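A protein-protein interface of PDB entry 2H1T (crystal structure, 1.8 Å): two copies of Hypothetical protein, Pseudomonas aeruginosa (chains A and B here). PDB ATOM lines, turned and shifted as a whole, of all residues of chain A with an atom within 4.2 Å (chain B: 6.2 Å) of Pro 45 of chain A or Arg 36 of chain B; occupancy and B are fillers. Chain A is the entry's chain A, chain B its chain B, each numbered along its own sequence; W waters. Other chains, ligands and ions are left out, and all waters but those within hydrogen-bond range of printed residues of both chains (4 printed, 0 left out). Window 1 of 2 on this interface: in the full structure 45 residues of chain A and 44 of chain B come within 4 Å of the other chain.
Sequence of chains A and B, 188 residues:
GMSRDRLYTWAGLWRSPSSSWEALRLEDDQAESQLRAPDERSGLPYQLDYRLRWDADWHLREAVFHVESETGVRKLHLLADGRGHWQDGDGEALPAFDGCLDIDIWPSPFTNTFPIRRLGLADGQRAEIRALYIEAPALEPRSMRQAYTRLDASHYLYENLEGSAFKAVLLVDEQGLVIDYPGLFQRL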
ATOM      1  N   ALA A  37     -26.623  -3.450  31.988  1.00  0.00           N
ATOM      2  CA  ALA A  37     -28.074  -3.396  31.917  1.00  0.00           C
ATOM      3  C   ALA A  37     -28.520  -2.771  30.598  1.00  0.00           C
ATOM      4  O   ALA A  37     -27.735  -2.112  29.914  1.00  0.00           O
ATOM      5  CB  ALA A  37     -28.658  -2.600  33.103  1.00  0.00           C
ATOM      6  N   LEU A  44     -30.774  -0.640  23.929  1.00  0.00           N
ATOM      7  CA  LEU A  44     -29.368  -0.911  23.727  1.00  0.00           C
ATOM      8  C   LEU A  44     -28.643  -0.932  25.083  1.00  0.00           C
ATOM      9  O   LEU A  44     -29.058  -0.270  26.043  1.00  0.00           O
ATOM     10  CB  LEU A  44     -28.736   0.129  22.798  1.00  0.00           C
ATOM     11  CG  LEU A  44     -29.400   0.235  21.405  1.00  0.00           C
ATOM     12  CD1 LEU A  44     -28.791   1.378  20.613  1.00  0.00           C
ATOM     13  CD2 LEU A  44     -29.256  -1.079  20.644  1.00  0.00           C
ATOM     14  N   PRO A  45     -27.576  -1.725  25.172  1.00  0.00           N
ATOM     15  CA  PRO A  45     -26.902  -1.921  26.461  1.00  0.00           C
ATOM     16  C   PRO A  45     -26.047  -0.766  26.950  1.00  0.00           C
ATOM     17  O   PRO A  45     -25.541   0.004  26.171  1.00  0.00           O
ATOM     18  CB  PRO A  45     -26.003  -3.146  26.212  1.00  0.00           C
ATOM     19  CG  PRO A  45     -25.752  -3.156  24.720  1.00  0.00           C
ATOM     20  CD  PRO A  45     -26.990  -2.535  24.090  1.00  0.00           C
ATOM     21  N   TYR A  46     -25.901  -0.647  28.258  1.00  0.00           N
ATOM     22  CA  TYR A  46     -24.889   0.237  28.817  1.00  0.00           C
ATOM     23  C   TYR A  46     -24.113  -0.493  29.908  1.00  0.00           C
ATOM     24  O   TYR A  46     -24.484  -1.582  30.353  1.00  0.00           O
ATOM     25  CB  TYR A  46     -25.519   1.556  29.330  1.00  0.00           C
ATOM     26  CG  TYR A  46     -26.471   1.380  30.483  1.00  0.00           C
ATOM     27  CD1 TYR A  46     -26.007   1.441  31.802  1.00  0.00           C
ATOM     28  CD2 TYR A  46     -27.850   1.175  30.276  1.00  0.00           C
ATOM     29  CE1 TYR A  46     -26.894   1.266  32.917  1.00  0.00           C
ATOM     30  CE2 TYR A  46     -28.743   0.974  31.403  1.00  0.00           C
ATOM     31  CZ  TYR A  46     -28.244   1.042  32.709  1.00  0.00           C
ATOM     32  OH  TYR A  46     -29.055   0.847  33.825  1.00  0.00           O
ATOM     33  N   GLN A  47     -22.982   0.085  30.281  1.00  0.00           N
ATOM     34  CA  GLN A  47     -22.256  -0.375  31.436  1.00  0.00           C
ATOM     35  C   GLN A  47     -21.979   0.838  32.311  1.00  0.00           C
ATOM     36  O   GLN A  47     -21.426   1.844  31.829  1.00  0.00           O
ATOM     37  CB  GLN A  47     -20.935  -1.034  31.086  1.00  0.00           C
ATOM     38  CG  GLN A  47     -20.159  -1.480  32.358  1.00  0.00           C
ATOM     39  CD  GLN A  47     -19.061  -2.495  32.095  1.00  0.00           C
ATOM     40  OE1 GLN A  47     -19.250  -3.452  31.325  1.00  0.00           O
ATOM     41  NE2 GLN A  47     -17.895  -2.293  32.730  1.00  0.00           N
ATOM     42  N   GLU A  68     -20.868   4.038  30.098  1.00  0.00           N
ATOM     43  CA  GLU A  68     -20.675   3.958  28.666  1.00  0.00           C
ATOM     44  C   GLU A  68     -21.888   3.330  27.975  1.00  0.00           C
ATOM     45  O   GLU A  68     -22.384   2.265  28.370  1.00  0.00           O
ATOM     46  CB  GLU A  68     -19.420   3.162  28.331  1.00  0.00           C
ATOM     47  CG  GLU A  68     -18.223   3.446  29.196  1.00  0.00           C
ATOM     48  CD  GLU A  68     -16.924   2.869  28.621  1.00  0.00           C
ATOM     49  OE1 GLU A  68     -16.975   2.008  27.687  1.00  0.00           O
ATOM     50  OE2 GLU A  68     -15.851   3.304  29.103  1.00  0.00           O
ATOM     51  N   SER A  69     -22.343   4.013  26.937  1.00  0.00           N
ATOM     52  CA  SER A  69     -23.513   3.623  26.180  1.00  0.00           C
ATOM     53  C   SER A  69     -23.318   4.069  24.745  1.00  0.00           C
ATOM     54  O   SER A  69     -22.307   4.672  24.408  1.00  0.00           O
ATOM     55  CB  SER A  69     -24.761   4.305  26.763  1.00  0.00           C
ATOM     56  OG  SER A  69     -24.748   5.714  26.511  1.00  0.00           O
ATOM     57  N   SER B  18     -34.078  -5.999  24.608  1.00  0.00           N
ATOM     58  CA  SER B  18     -32.787  -5.415  24.316  1.00  0.00           C
ATOM     59  C   SER B  18     -32.060  -6.109  23.168  1.00  0.00           C
ATOM     60  O   SER B  18     -32.506  -7.104  22.659  1.00  0.00           O
ATOM     61  CB  SER B  18     -31.919  -5.302  25.593  1.00  0.00           C
ATOM     62  OG  SER B  18     -31.289  -6.526  25.978  1.00  0.00           O
ATOM     63  N   SER B  19     -30.932  -5.536  22.797  1.00  0.00           N
ATOM     64  CA  SER B  19     -30.175  -5.987  21.673  1.00  0.00           C
ATOM     65  C   SER B  19     -28.700  -5.719  21.842  1.00  0.00           C
ATOM     66  O   SER B  19     -28.213  -5.411  22.942  1.00  0.00           O
ATOM     67  CB  SER B  19     -30.722  -5.345  20.404  1.00  0.00           C
ATOM     68  OG  SER B  19     -30.328  -6.124  19.287  1.00  0.00           O
ATOM     69  N   SER B  20     -27.989  -5.878  20.742  1.00  0.00           N
ATOM     70  CA  SER B  20     -26.565  -5.686  20.670  1.00  0.00           C
ATOM     71  C   SER B  20     -26.157  -4.253  20.364  1.00  0.00           C
ATOM     72  O   SER B  20     -26.867  -3.518  19.671  1.00  0.00           O
ATOM     73  CB  SER B  20     -25.985  -6.624  19.613  1.00  0.00           C
ATOM     74  OG  SER B  20     -26.555  -6.400  18.316  1.00  0.00           O
ATOM     75  N   TRP B  21     -24.986  -3.888  20.878  1.00  0.00           N
ATOM     76  CA  TRP B  21     -24.317  -2.657  20.481  1.00  0.00           C
ATOM     77  C   TRP B  21     -22.860  -3.017  20.284  1.00  0.00           C
ATOM     78  O   TRP B  21     -22.288  -3.607  21.152  1.00  0.00           O
ATOM     79  CB  TRP B  21     -24.510  -1.570  21.523  1.00  0.00           C
ATOM     80  CG  TRP B  21     -23.535  -0.433  21.423  1.00  0.00           C
ATOM     81  CD1 TRP B  21     -23.185   0.267  20.313  1.00  0.00           C
ATOM     82  CD2 TRP B  21     -22.786   0.104  22.496  1.00  0.00           C
ATOM     83  NE1 TRP B  21     -22.234   1.232  20.623  1.00  0.00           N
ATOM     84  CE2 TRP B  21     -21.971   1.153  21.963  1.00  0.00           C
ATOM     85  CE3 TRP B  21     -22.767  -0.142  23.892  1.00  0.00           C
ATOM     86  CZ2 TRP B  21     -21.115   1.922  22.769  1.00  0.00           C
ATOM     87  CZ3 TRP B  21     -21.897   0.616  24.696  1.00  0.00           C
ATOM     88  CH2 TRP B  21     -21.074   1.625  24.127  1.00  0.00           C
ATOM     89  N   GLU B  22     -22.330  -2.701  19.088  1.00  0.00           N
ATOM     90  CA  GLU B  22     -20.964  -3.022  18.703  1.00  0.00           C
ATOM     91  C   GLU B  22     -20.222  -1.797  18.187  1.00  0.00           C
ATOM     92  O   GLU B  22     -20.715  -1.043  17.308  1.00  0.00           O
ATOM     93  CB  GLU B  22     -20.950  -4.124  17.642  1.00  0.00           C
ATOM     94  CG  GLU B  22     -19.537  -4.466  17.215  1.00  0.00           C
ATOM     95  CD  GLU B  22     -19.400  -5.714  16.348  1.00  0.00           C
ATOM     96  OE1 GLU B  22     -20.385  -6.169  15.749  1.00  0.00           O
ATOM     97  OE2 GLU B  22     -18.245  -6.255  16.304  1.00  0.00           O
ATOM     98  N   GLN B  34     -15.625  -4.218  20.527  1.00  0.00           N
ATOM     99  CA  GLN B  34     -16.306  -4.393  21.801  1.00  0.00           C
ATOM    100  C   GLN B  34     -17.782  -4.443  21.512  1.00  0.00           C
ATOM    101  O   GLN B  34     -18.334  -3.479  21.005  1.00  0.00           O
ATOM    102  CB  GLN B  34     -15.999  -3.210  22.693  1.00  0.00           C
ATOM    103  CG  GLN B  34     -16.666  -3.316  24.031  1.00  0.00           C
ATOM    104  CD  GLN B  34     -15.936  -2.506  25.060  1.00  0.00           C
ATOM    105  OE1 GLN B  34     -15.445  -3.053  26.045  1.00  0.00           O
ATOM    106  NE2 GLN B  34     -15.803  -1.204  24.814  1.00  0.00           N
ATOM    107  N   LEU B  35     -18.389  -5.556  21.888  1.00  0.00           N
ATOM    108  CA  LEU B  35     -19.742  -5.914  21.558  1.00  0.00           C
ATOM    109  C   LEU B  35     -20.420  -6.220  22.916  1.00  0.00           C
ATOM    110  O   LEU B  35     -19.913  -7.039  23.717  1.00  0.00           O
ATOM    111  CB  LEU B  35     -19.703  -7.118  20.613  1.00  0.00           C
ATOM    112  CG  LEU B  35     -21.006  -7.706  20.091  1.00  0.00           C
ATOM    113  CD1 LEU B  35     -20.683  -8.462  18.823  1.00  0.00           C
ATOM    114  CD2 LEU B  35     -21.684  -8.578  21.114  1.00  0.00           C
ATOM    115  N   ARG B  36     -21.506  -5.512  23.199  1.00  0.00           N
ATOM    116  CA  ARG B  36     -22.333  -5.765  24.366  1.00  0.00           C
ATOM    117  C   ARG B  36     -23.702  -6.254  23.901  1.00  0.00           C
ATOM    118  O   ARG B  36     -24.300  -5.688  22.971  1.00  0.00           O
ATOM    119  CB  ARG B  36     -22.504  -4.466  25.134  1.00  0.00           C
ATOM    120  CG  ARG B  36     -21.173  -3.952  25.651  1.00  0.00           C
ATOM    121  CD  ARG B  36     -21.165  -2.488  26.019  1.00  0.00           C
ATOM    122  NE  ARG B  36     -20.163  -2.289  27.061  1.00  0.00           N
ATOM    123  CZ  ARG B  36     -19.288  -1.284  27.183  1.00  0.00           C
ATOM    124  NH1 ARG B  36     -19.200  -0.274  26.333  1.00  0.00           N
ATOM    125  NH2 ARG B  36     -18.446  -1.330  28.199  1.00  0.00           N
ATOM    126  N   ALA B  37     -24.226  -7.284  24.547  1.00  0.00           N
ATOM    127  CA  ALA B  37     -25.490  -7.891  24.107  1.00  0.00           C
ATOM    128  C   ALA B  37     -26.091  -8.732  25.214  1.00  0.00           C
ATOM    129  O   ALA B  37     -25.384  -9.082  26.158  1.00  0.00           O
ATOM    130  CB  ALA B  37     -25.262  -8.764  22.847  1.00  0.00           C
ATOM    131  N   PRO B  38     -27.409  -9.015  25.131  1.00  0.00           N
ATOM    132  CA  PRO B  38     -28.011  -9.939  26.079  1.00  0.00           C
ATOM    133  C   PRO B  38     -27.807 -11.392  25.667  1.00  0.00           C
ATOM    134  O   PRO B  38     -27.868 -11.744  24.469  1.00  0.00           O
ATOM    135  CB  PRO B  38     -29.515  -9.596  26.007  1.00  0.00           C
ATOM    136  CG  PRO B  38     -29.716  -9.091  24.589  1.00  0.00           C
ATOM    137  CD  PRO B  38     -28.395  -8.491  24.178  1.00  0.00           C
ATOM    138  N   PRO B  45     -26.822  -9.681  30.619  1.00  0.00           N
ATOM    139  CA  PRO B  45     -25.893  -9.130  29.642  1.00  0.00           C
ATOM    140  C   PRO B  45     -24.478  -9.762  29.621  1.00  0.00           C
ATOM    141  O   PRO B  45     -23.991 -10.340  30.580  1.00  0.00           O
ATOM    142  CB  PRO B  45     -25.841  -7.659  30.003  1.00  0.00           C
ATOM    143  CG  PRO B  45     -26.224  -7.579  31.429  1.00  0.00           C
ATOM    144  CD  PRO B  45     -26.884  -8.847  31.836  1.00  0.00           C
ATOM    145  N   TYR B  46     -23.843  -9.690  28.467  1.00  0.00           N
ATOM    146  CA  TYR B  46     -22.442 -10.066  28.377  1.00  0.00           C
ATOM    147  C   TYR B  46     -21.705  -9.024  27.569  1.00  0.00           C
ATOM    148  O   TYR B  46     -22.314  -8.148  26.893  1.00  0.00           O
ATOM    149  CB  TYR B  46     -22.254 -11.494  27.800  1.00  0.00           C
ATOM    150  CG  TYR B  46     -22.739 -11.648  26.352  1.00  0.00           C
ATOM    151  CD1 TYR B  46     -21.921 -11.295  25.292  1.00  0.00           C
ATOM    152  CD2 TYR B  46     -23.998 -12.152  26.072  1.00  0.00           C
ATOM    153  CE1 TYR B  46     -22.359 -11.410  23.964  1.00  0.00           C
ATOM    154  CE2 TYR B  46     -24.437 -12.299  24.766  1.00  0.00           C
ATOM    155  CZ  TYR B  46     -23.607 -11.907  23.708  1.00  0.00           C
ATOM    156  OH  TYR B  46     -24.008 -12.018  22.399  1.00  0.00           O
ATOM    157  N   GLN B  47     -20.384  -9.085  27.680  1.00  0.00           N
ATOM    158  CA  GLN B  47     -19.548  -8.258  26.844  1.00  0.00           C
ATOM    159  C   GLN B  47     -18.542  -9.120  26.159  1.00  0.00           C
ATOM    160  O   GLN B  47     -17.849  -9.864  26.805  1.00  0.00           O
ATOM    161  CB  GLN B  47     -18.821  -7.211  27.612  1.00  0.00           C
ATOM    162  CG  GLN B  47     -17.987  -6.352  26.681  1.00  0.00           C
ATOM    163  CD  GLN B  47     -17.550  -5.106  27.339  1.00  0.00           C
ATOM    164  OE1 GLN B  47     -18.386  -4.339  27.831  1.00  0.00           O
ATOM    165  NE2 GLN B  47     -16.231  -4.887  27.394  1.00  0.00           N
ATOM    166  N   LEU B  48     -18.436  -8.965  24.849  1.00  0.00           N
ATOM    167  CA  LEU B  48     -17.482  -9.722  24.061  1.00  0.00           C
ATOM    168  C   LEU B  48     -16.476  -8.712  23.495  1.00  0.00           C
ATOM    169  O   LEU B  48     -16.869  -7.779  22.837  1.00  0.00           O
ATOM    170  CB  LEU B  48     -18.198 -10.399  22.886  1.00  0.00           C
ATOM    171  CG  LEU B  48     -17.213 -11.037  21.881  1.00  0.00           C
ATOM    172  CD1 LEU B  48     -16.472 -12.204  22.522  1.00  0.00           C
ATOM    173  CD2 LEU B  48     -17.936 -11.509  20.609  1.00  0.00           C
HETATM  174  O   HOH W   1     -15.081   0.691  26.659  1.00  0.00           O
HETATM  175  O   HOH W   2     -20.476  -4.083  29.086  1.00  0.00           O
HETATM  176  O   HOH W   3     -16.970  -4.403  30.475  1.00  0.00           O
HETATM  177  O   HOH W   4     -17.740   0.217  30.370  1.00  0.00           O
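Gln 47 of chain B touches its own counterpart, Gln 47 of chain A.
Of the 8 pairs that touch across the chains among the printed residues, 1 has its exchanged pair printed and touching as well.
Among the printed residues, merely in contact across the chains: Ser 69 of chain A with Trp 21 of chain B (3.3 Å), Pro 45 of chain A with Ser 19 of chain B (3.3 Å), Pro 45 of chain A with Arg 36 of chain B (3.4 Å), Leu 44 of chain A with Ser 20 of chain B (3.6 Å), Pro 45 of chain A with Trp 21 of chain B (3.6 Å), Gln 47 of chain A with Gln 47 of chain B (3.7 Å) and Gln 47 of chain A with Arg 36 of chain B (3.8 Å).
Of chain A, only Pro 45, Gln 47 and Glu 68 come within 4 Å of Arg 36 of chain B.
Printed residues of chain B within 4 Å of Glu 68 of chain A: Arg 36 (3.5 Å).
Of the printed residues of chain A, Ser 19 of chain B touches Pro 45.
Gln 34 of chain B touches none of the printed residues of chain A.
Ala 37 of chain A touches none of the printed residues of chain B.
O of Gln 47 of chain A lies within hydrogen-bond range of N of Glu 68 of chain A (2.8 Å).
O of Arg 36 of chain B is in hydrogen-bond range of N of Trp 21 of chain B (2.8 Å).
The side-chain amide oxygen (OE1) of Gln 34 of chain B sits at hydrogen-bond distance from the side-chain amide nitrogen (NE2) of Gln 47 of chain B, 2.4 Å away.
The side-chain amide oxygen (OE1) of Gln 47 of chain B is in hydrogen-bond range of the guanidinium group (NE) of Arg 36 of chain B (2.8 Å).
Printed residues of chain A that touch a printed residue of chain B: Leu 44, Pro 45, Gln 47, Glu 68 and Ser 69.
Hydrophobic or aromatic side chains of chain A that line the printed part of chain B: Leu 44 and Pro 45.
Of the 14 printed residues of chain B, 5 touch a printed residue of chain A.
Hydrophobic or aromatic side chains of chain B within 4 Å of the printed part of chain A: Trp 21.
Along chain B the printed residues that touch a printed residue of chain A span positions 19 to 47.
Among the printed residues, 8 pairs touch across the chains.
Water W2 lies within hydrogen-bond range of OE1 of Gln 47 of chain B (2.5 Å), OE1 of Gln 47 of chain A (2.6 Å) and NE of Arg 36 of chain B (2.7 Å).
Water W1 lies within hydrogen-bond range of the side-chain carboxylate of Glu 68 of chain A (2.5 Å) and the side-chain amide nitrogen of Gln 34 of chain B (2.7 Å).
Water W3 lies within hydrogen-bond range of the side-chain amide oxygen of Gln 47 of chain A (2.6 Å) and the side-chain amide oxygen of Gln 47 of chain B (3.0 Å).
Water W4 lies within hydrogen-bond range of the guanidinium group (NH2) of Arg 36 of chain B, the side-chain carboxylate (OE1) of Glu 68 of chain A and the side-chain amide nitrogen (NE2) of Gln 47 of chain A.
The side-chain carboxylate (OE1) of Glu 68 of chain A lies within salt-bridge range of the guanidinium group (NH1) of Arg 36 of chain B (3.5 Å).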
